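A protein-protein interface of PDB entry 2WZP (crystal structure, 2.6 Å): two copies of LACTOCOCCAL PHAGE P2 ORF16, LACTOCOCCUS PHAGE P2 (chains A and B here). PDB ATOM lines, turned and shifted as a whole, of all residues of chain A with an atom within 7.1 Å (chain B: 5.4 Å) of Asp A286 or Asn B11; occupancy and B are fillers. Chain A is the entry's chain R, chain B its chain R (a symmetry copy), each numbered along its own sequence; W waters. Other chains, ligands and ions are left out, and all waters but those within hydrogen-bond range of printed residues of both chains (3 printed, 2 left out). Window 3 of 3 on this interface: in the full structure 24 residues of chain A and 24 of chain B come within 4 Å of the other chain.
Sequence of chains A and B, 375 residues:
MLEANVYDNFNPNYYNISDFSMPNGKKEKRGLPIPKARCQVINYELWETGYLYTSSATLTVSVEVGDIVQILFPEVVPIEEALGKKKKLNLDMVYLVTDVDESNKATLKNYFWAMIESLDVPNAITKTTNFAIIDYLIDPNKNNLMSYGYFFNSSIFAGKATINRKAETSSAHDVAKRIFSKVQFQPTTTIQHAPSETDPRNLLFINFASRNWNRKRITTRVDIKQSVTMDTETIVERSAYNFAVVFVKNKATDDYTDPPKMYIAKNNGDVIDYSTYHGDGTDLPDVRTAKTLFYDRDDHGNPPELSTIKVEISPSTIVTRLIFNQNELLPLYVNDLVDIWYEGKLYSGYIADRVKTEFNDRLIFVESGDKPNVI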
ATOM      1  N   ASN A 242      27.193  15.785  35.379  1.00  0.00           N
ATOM      2  CA  ASN A 242      26.265  16.524  34.521  1.00  0.00           C
ATOM      3  C   ASN A 242      24.831  15.955  34.499  1.00  0.00           C
ATOM      4  O   ASN A 242      23.972  16.464  33.795  1.00  0.00           O
ATOM      5  CB  ASN A 242      26.850  16.597  33.115  1.00  0.00           C
ATOM      6  CG  ASN A 242      27.052  15.301  32.387  1.00  0.00           C
ATOM      7  OD1 ASN A 242      26.275  14.350  32.528  1.00  0.00           O
ATOM      8  ND2 ASN A 242      28.047  15.277  31.492  1.00  0.00           N
ATOM      9  N   ASN A 267      23.965  22.051  27.950  1.00  0.00           N
ATOM     10  CA  ASN A 267      25.190  22.849  27.756  1.00  0.00           C
ATOM     11  C   ASN A 267      25.129  24.297  28.275  1.00  0.00           C
ATOM     12  O   ASN A 267      26.136  24.807  28.757  1.00  0.00           O
ATOM     13  CB  ASN A 267      25.595  22.841  26.302  1.00  0.00           C
ATOM     14  CG  ASN A 267      26.127  21.515  25.829  1.00  0.00           C
ATOM     15  OD1 ASN A 267      26.089  21.211  24.635  1.00  0.00           O
ATOM     16  ND2 ASN A 267      26.675  20.722  26.736  1.00  0.00           N
ATOM     17  N   GLY A 281      19.760  16.425  20.953  1.00  0.00           N
ATOM     18  CA  GLY A 281      20.961  15.924  21.612  1.00  0.00           C
ATOM     19  C   GLY A 281      22.210  16.739  21.389  1.00  0.00           C
ATOM     20  O   GLY A 281      23.231  16.458  22.005  1.00  0.00           O
ATOM     21  N   LEU A 284      23.136  18.951  24.645  1.00  0.00           N
ATOM     22  CA  LEU A 284      23.498  18.240  25.880  1.00  0.00           C
ATOM     23  C   LEU A 284      25.013  17.877  25.897  1.00  0.00           C
ATOM     24  O   LEU A 284      25.587  17.663  24.831  1.00  0.00           O
ATOM     25  CB  LEU A 284      22.691  16.937  26.022  1.00  0.00           C
ATOM     26  CG  LEU A 284      21.175  17.009  26.063  1.00  0.00           C
ATOM     27  CD1 LEU A 284      20.566  15.613  26.035  1.00  0.00           C
ATOM     28  CD2 LEU A 284      20.682  17.859  27.245  1.00  0.00           C
ATOM     29  N   PRO A 285      25.663  17.729  27.071  1.00  0.00           N
ATOM     30  CA  PRO A 285      27.079  17.308  27.080  1.00  0.00           C
ATOM     31  C   PRO A 285      27.343  16.030  26.265  1.00  0.00           C
ATOM     32  O   PRO A 285      26.472  15.158  26.131  1.00  0.00           O
ATOM     33  CB  PRO A 285      27.369  17.120  28.565  1.00  0.00           C
ATOM     34  CG  PRO A 285      26.471  18.100  29.229  1.00  0.00           C
ATOM     35  CD  PRO A 285      25.181  17.951  28.450  1.00  0.00           C
ATOM     36  N   ASP A 286      28.543  15.966  25.662  1.00  0.00           N
ATOM     37  CA  ASP A 286      28.967  14.904  24.759  1.00  0.00           C
ATOM     38  C   ASP A 286      29.348  13.571  25.410  1.00  0.00           C
ATOM     39  O   ASP A 286      29.631  12.584  24.707  1.00  0.00           O
ATOM     40  CB  ASP A 286      29.926  15.410  23.654  1.00  0.00           C
ATOM     41  CG  ASP A 286      31.356  15.763  24.041  1.00  0.00           C
ATOM     42  OD1 ASP A 286      31.675  15.748  25.269  1.00  0.00           O
ATOM     43  OD2 ASP A 286      32.156  16.091  23.124  1.00  0.00           O
ATOM     44  N   VAL A 287      29.260  13.527  26.752  1.00  0.00           N
ATOM     45  CA  VAL A 287      29.402  12.322  27.580  1.00  0.00           C
ATOM     46  C   VAL A 287      28.423  12.507  28.760  1.00  0.00           C
ATOM     47  O   VAL A 287      28.186  13.653  29.150  1.00  0.00           O
ATOM     48  CB  VAL A 287      30.849  12.040  28.130  1.00  0.00           C
ATOM     49  CG1 VAL A 287      31.851  11.711  27.044  1.00  0.00           C
ATOM     50  CG2 VAL A 287      31.352  13.138  29.064  1.00  0.00           C
ATOM     51  N   ARG A 288      27.967  11.403  29.393  1.00  0.00           N
ATOM     52  CA  ARG A 288      27.129  11.501  30.594  1.00  0.00           C
ATOM     53  C   ARG A 288      27.941  11.101  31.835  1.00  0.00           C
ATOM     54  O   ARG A 288      28.632  10.085  31.825  1.00  0.00           O
ATOM     55  CB  ARG A 288      25.883  10.624  30.469  1.00  0.00           C
ATOM     56  CG  ARG A 288      24.991  10.671  31.708  1.00  0.00           C
ATOM     57  CD  ARG A 288      23.779   9.814  31.551  1.00  0.00           C
ATOM     58  NE  ARG A 288      22.887  10.337  30.513  1.00  0.00           N
ATOM     59  CZ  ARG A 288      21.866   9.653  30.022  1.00  0.00           C
ATOM     60  NH1 ARG A 288      21.614   8.421  30.451  1.00  0.00           N
ATOM     61  NH2 ARG A 288      21.119  10.170  29.066  1.00  0.00           N
ATOM     62  N   THR A 289      27.854  11.900  32.904  1.00  0.00           N
ATOM     63  CA  THR A 289      28.569  11.691  34.182  1.00  0.00           C
ATOM     64  C   THR A 289      27.514  11.760  35.299  1.00  0.00           C
ATOM     65  O   THR A 289      27.236  12.823  35.839  1.00  0.00           O
ATOM     66  CB  THR A 289      29.716  12.680  34.293  1.00  0.00           C
ATOM     67  OG1 THR A 289      29.195  13.954  33.988  1.00  0.00           O
ATOM     68  CG2 THR A 289      30.838  12.406  33.291  1.00  0.00           C
ATOM     69  N   SER A 316      29.415  19.964  32.132  1.00  0.00           N
ATOM     70  CA  SER A 316      30.788  19.495  32.238  1.00  0.00           C
ATOM     71  C   SER A 316      30.885  18.080  31.727  1.00  0.00           C
ATOM     72  O   SER A 316      29.851  17.439  31.533  1.00  0.00           O
ATOM     73  CB  SER A 316      31.224  19.445  33.698  1.00  0.00           C
ATOM     74  OG  SER A 316      30.230  18.848  34.512  1.00  0.00           O
ATOM     75  N   THR A 317      32.119  17.615  31.423  1.00  0.00           N
ATOM     76  CA  THR A 317      32.418  16.261  30.898  1.00  0.00           C
ATOM     77  C   THR A 317      33.339  15.486  31.826  1.00  0.00           C
ATOM     78  O   THR A 317      33.246  15.671  33.051  1.00  0.00           O
ATOM     79  CB  THR A 317      32.955  16.359  29.436  1.00  0.00           C
ATOM     80  OG1 THR A 317      34.112  17.198  29.343  1.00  0.00           O
ATOM     81  CG2 THR A 317      31.880  16.766  28.428  1.00  0.00           C
ATOM     82  N   ILE A 318      34.186  14.576  31.256  1.00  0.00           N
ATOM     83  CA  ILE A 318      35.215  13.829  31.978  1.00  0.00           C
ATOM     84  C   ILE A 318      36.269  14.897  32.244  1.00  0.00           C
ATOM     85  O   ILE A 318      36.675  15.603  31.333  1.00  0.00           O
ATOM     86  CB  ILE A 318      35.788  12.600  31.193  1.00  0.00           C
ATOM     87  CG1 ILE A 318      34.740  11.490  31.046  1.00  0.00           C
ATOM     88  CG2 ILE A 318      37.040  12.038  31.912  1.00  0.00           C
ATOM     89  CD1 ILE A 318      35.040  10.465  29.962  1.00  0.00           C
ATOM     90  N   ASN B   9      32.482   8.132  21.982  1.00  0.00           N
ATOM     91  CA  ASN B   9      31.714   7.663  23.120  1.00  0.00           C
ATOM     92  C   ASN B   9      30.263   7.345  22.733  1.00  0.00           C
ATOM     93  O   ASN B   9      29.630   8.129  22.012  1.00  0.00           O
ATOM     94  CB  ASN B   9      31.717   8.733  24.221  1.00  0.00           C
ATOM     95  CG  ASN B   9      31.093   8.241  25.493  1.00  0.00           C
ATOM     96  OD1 ASN B   9      29.976   8.598  25.850  1.00  0.00           O
ATOM     97  ND2 ASN B   9      31.771   7.339  26.162  1.00  0.00           N
ATOM     98  N   PHE B  10      29.722   6.206  23.233  1.00  0.00           N
ATOM     99  CA  PHE B  10      28.311   5.849  23.039  1.00  0.00           C
ATOM    100  C   PHE B  10      27.526   6.590  24.126  1.00  0.00           C
ATOM    101  O   PHE B  10      27.078   6.002  25.110  1.00  0.00           O
ATOM    102  CB  PHE B  10      28.122   4.353  23.163  1.00  0.00           C
ATOM    103  CG  PHE B  10      28.723   3.527  22.050  1.00  0.00           C
ATOM    104  CD1 PHE B  10      29.100   4.112  20.855  1.00  0.00           C
ATOM    105  CD2 PHE B  10      28.885   2.147  22.198  1.00  0.00           C
ATOM    106  CE1 PHE B  10      29.655   3.344  19.843  1.00  0.00           C
ATOM    107  CE2 PHE B  10      29.426   1.377  21.179  1.00  0.00           C
ATOM    108  CZ  PHE B  10      29.791   1.973  20.005  1.00  0.00           C
ATOM    109  N   ASN B  11      27.422   7.921  23.943  1.00  0.00           N
ATOM    110  CA  ASN B  11      26.783   8.875  24.832  1.00  0.00           C
ATOM    111  C   ASN B  11      25.254   8.712  24.817  1.00  0.00           C
ATOM    112  O   ASN B  11      24.620   8.993  23.775  1.00  0.00           O
ATOM    113  CB  ASN B  11      27.205  10.290  24.414  1.00  0.00           C
ATOM    114  CG  ASN B  11      26.571  11.398  25.191  1.00  0.00           C
ATOM    115  OD1 ASN B  11      26.148  11.199  26.315  1.00  0.00           O
ATOM    116  ND2 ASN B  11      26.425  12.584  24.574  1.00  0.00           N
ATOM    117  N   PRO B  12      24.648   8.269  25.975  1.00  0.00           N
ATOM    118  CA  PRO B  12      23.174   8.125  26.024  1.00  0.00           C
ATOM    119  C   PRO B  12      22.444   9.449  25.822  1.00  0.00           C
ATOM    120  O   PRO B  12      21.353   9.465  25.267  1.00  0.00           O
ATOM    121  CB  PRO B  12      22.909   7.481  27.380  1.00  0.00           C
ATOM    122  CG  PRO B  12      24.149   7.702  28.179  1.00  0.00           C
ATOM    123  CD  PRO B  12      25.282   7.872  27.253  1.00  0.00           C
ATOM    124  N   ASN B  13      23.084  10.582  26.183  1.00  0.00           N
ATOM    125  CA  ASN B  13      22.491  11.894  25.964  1.00  0.00           C
ATOM    126  C   ASN B  13      22.151  12.060  24.511  1.00  0.00           C
ATOM    127  O   ASN B  13      21.114  12.633  24.214  1.00  0.00           O
ATOM    128  CB  ASN B  13      23.443  12.984  26.407  1.00  0.00           C
ATOM    129  CG  ASN B  13      23.562  13.121  27.894  1.00  0.00           C
ATOM    130  OD1 ASN B  13      22.822  12.495  28.677  1.00  0.00           O
ATOM    131  ND2 ASN B  13      24.472  13.988  28.314  1.00  0.00           N
ATOM    132  N   TYR B  14      22.968  11.463  23.609  1.00  0.00           N
ATOM    133  CA  TYR B  14      22.805  11.531  22.164  1.00  0.00           C
ATOM    134  C   TYR B  14      21.949  10.428  21.584  1.00  0.00           C
ATOM    135  O   TYR B  14      21.041  10.718  20.808  1.00  0.00           O
ATOM    136  CB  TYR B  14      24.175  11.566  21.474  1.00  0.00           C
ATOM    137  CG  TYR B  14      24.069  11.868  19.999  1.00  0.00           C
ATOM    138  CD1 TYR B  14      23.889  13.170  19.545  1.00  0.00           C
ATOM    139  CD2 TYR B  14      24.054  10.841  19.058  1.00  0.00           C
ATOM    140  CE1 TYR B  14      23.727  13.445  18.189  1.00  0.00           C
ATOM    141  CE2 TYR B  14      23.865  11.101  17.706  1.00  0.00           C
ATOM    142  CZ  TYR B  14      23.722  12.406  17.268  1.00  0.00           C
ATOM    143  OH  TYR B  14      23.547  12.641  15.909  1.00  0.00           O
ATOM    144  N   TYR B  15      22.246   9.168  21.928  1.00  0.00           N
ATOM    145  CA  TYR B  15      21.554   7.999  21.401  1.00  0.00           C
ATOM    146  C   TYR B  15      20.223   7.647  22.022  1.00  0.00           C
ATOM    147  O   TYR B  15      19.408   6.990  21.363  1.00  0.00           O
ATOM    148  CB  TYR B  15      22.492   6.799  21.376  1.00  0.00           C
ATOM    149  CG  TYR B  15      23.674   7.034  20.467  1.00  0.00           C
ATOM    150  CD1 TYR B  15      24.931   7.347  20.989  1.00  0.00           C
ATOM    151  CD2 TYR B  15      23.520   7.047  19.081  1.00  0.00           C
ATOM    152  CE1 TYR B  15      26.012   7.633  20.152  1.00  0.00           C
ATOM    153  CE2 TYR B  15      24.584   7.369  18.235  1.00  0.00           C
ATOM    154  CZ  TYR B  15      25.833   7.640  18.775  1.00  0.00           C
ATOM    155  OH  TYR B  15      26.881   7.929  17.936  1.00  0.00           O
ATOM    156  N   ASN B  16      19.958   8.105  23.251  1.00  0.00           N
ATOM    157  CA  ASN B  16      18.706   7.779  23.928  1.00  0.00           C
ATOM    158  C   ASN B  16      17.533   8.678  23.504  1.00  0.00           C
ATOM    159  O   ASN B  16      16.753   9.160  24.318  1.00  0.00           O
ATOM    160  CB  ASN B  16      18.938   7.727  25.437  1.00  0.00           C
ATOM    161  CG  ASN B  16      17.930   6.953  26.221  1.00  0.00           C
ATOM    162  OD1 ASN B  16      17.536   5.843  25.873  1.00  0.00           O
ATOM    163  ND2 ASN B  16      17.509   7.531  27.314  1.00  0.00           N
ATOM    164  N   ASN B 144      25.702   5.892  32.279  1.00  0.00           N
ATOM    165  CA  ASN B 144      26.717   6.743  31.681  1.00  0.00           C
ATOM    166  C   ASN B 144      26.973   6.334  30.237  1.00  0.00           C
ATOM    167  O   ASN B 144      27.373   7.181  29.429  1.00  0.00           O
ATOM    168  CB  ASN B 144      28.016   6.645  32.503  1.00  0.00           C
ATOM    169  CG  ASN B 144      28.049   7.554  33.697  1.00  0.00           C
ATOM    170  OD1 ASN B 144      27.132   8.343  33.932  1.00  0.00           O
ATOM    171  ND2 ASN B 144      29.125   7.497  34.457  1.00  0.00           N
ATOM    172  N   MET B 146      25.482   4.036  26.680  1.00  0.00           N
ATOM    173  CA  MET B 146      24.298   3.581  25.949  1.00  0.00           C
ATOM    174  C   MET B 146      24.180   2.059  25.913  1.00  0.00           C
ATOM    175  O   MET B 146      25.184   1.347  25.919  1.00  0.00           O
ATOM    176  CB  MET B 146      24.299   4.189  24.509  1.00  0.00           C
ATOM    177  CG  MET B 146      23.006   4.010  23.698  1.00  0.00           C
ATOM    178  SD  MET B 146      21.579   4.630  24.579  1.00  0.00           S
ATOM    179  CE  MET B 146      20.325   4.238  23.532  1.00  0.00           C
HETATM  180  O   HOH W   1      28.853   8.989  28.278  1.00  0.00           O
HETATM  181  O   HOH W   2      28.019  12.559  22.076  1.00  0.00           O
HETATM  182  O   HOH W   3      24.435  15.671  30.877  1.00  0.00           O
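The side-chain amide oxygen (OD1) of Asn B144 lies close to the backbone carbonyl oxygen (O) of Arg A288 (3.1 Å). The backbone carbonyl oxygen of Asp A286 lies close to the side-chain amide nitrogen of Asn B11 (3.2 Å). O of Pro A285 sits at hydrogen-bond distance from ND2 of Asn B11. The backbone carbonyl oxygen (O) of Pro A285 is in hydrogen-bond range of the side-chain amide nitrogen (ND2) of Asn B13 (3.2 Å). The side-chain amide oxygen (OD1) of Asn B13 lies within hydrogen-bond range of the guanidinium group (NE) of Arg A288, 2.8 Å away.
The side-chain amide nitrogen of Asn A242 is in hydrogen-bond range of the backbone carbonyl oxygen of Val A287 (2.9 Å). The side-chain amide oxygen (OD1) of Asn B9 lies close to the backbone NH (N) of Asn B11. The side-chain amide oxygen of Asn A242 lies within hydrogen-bond range of the backbone NH of Thr A289 (2.9 Å). N of Asn B13 lies within hydrogen-bond range of OD1 of Asn B11 (3.1 Å).
CD1 of Leu A284 touches O of Asn B13, at 3.5 Å. Val A287 touches Asn B9 (CG1 to OD1, 3.8 Å). Val A287 touches Asn B11. ND2 of Asn B13 touches O of Val A287 (3.8 Å). Arg A288 touches Asn B11 (N to OD1, 3.6 Å). CB of Pro B12 touches NH1 of Arg A288, at 3.5 Å. Thr A289 touches Asn B144.
Of the printed residues of chain A, Asn B9 touches Val A287. Of the printed residues of chain A, Pro B12 touches Arg A288. Tyr B15 touches none of the printed residues of chain A. Gly A281 touches none of the printed residues of chain B. The nearest residue of chain B that does not touch Asp A286 is Asn B9 (4.2 Å).
Among the printed residues, no Asp or Glu carboxylate lies within 4 Å of a Lys or Arg side-chain nitrogen of the other chain.
No position is printed for both chains.
Water W1 lies within hydrogen-bond range of O of Asn B144 (2.6 Å), OD1 of Asn B9 (2.7 Å) and N of Arg A288 (2.8 Å). Water W3 bridges the side-chain amide oxygen (OD1) of Asn A242 and the side-chain amide nitrogen (ND2) of Asn B13. Water W2 lies within hydrogen-bond range of ND2 of Asn B11 (3.0 Å) and O of Asp A286 (3.1 Å).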
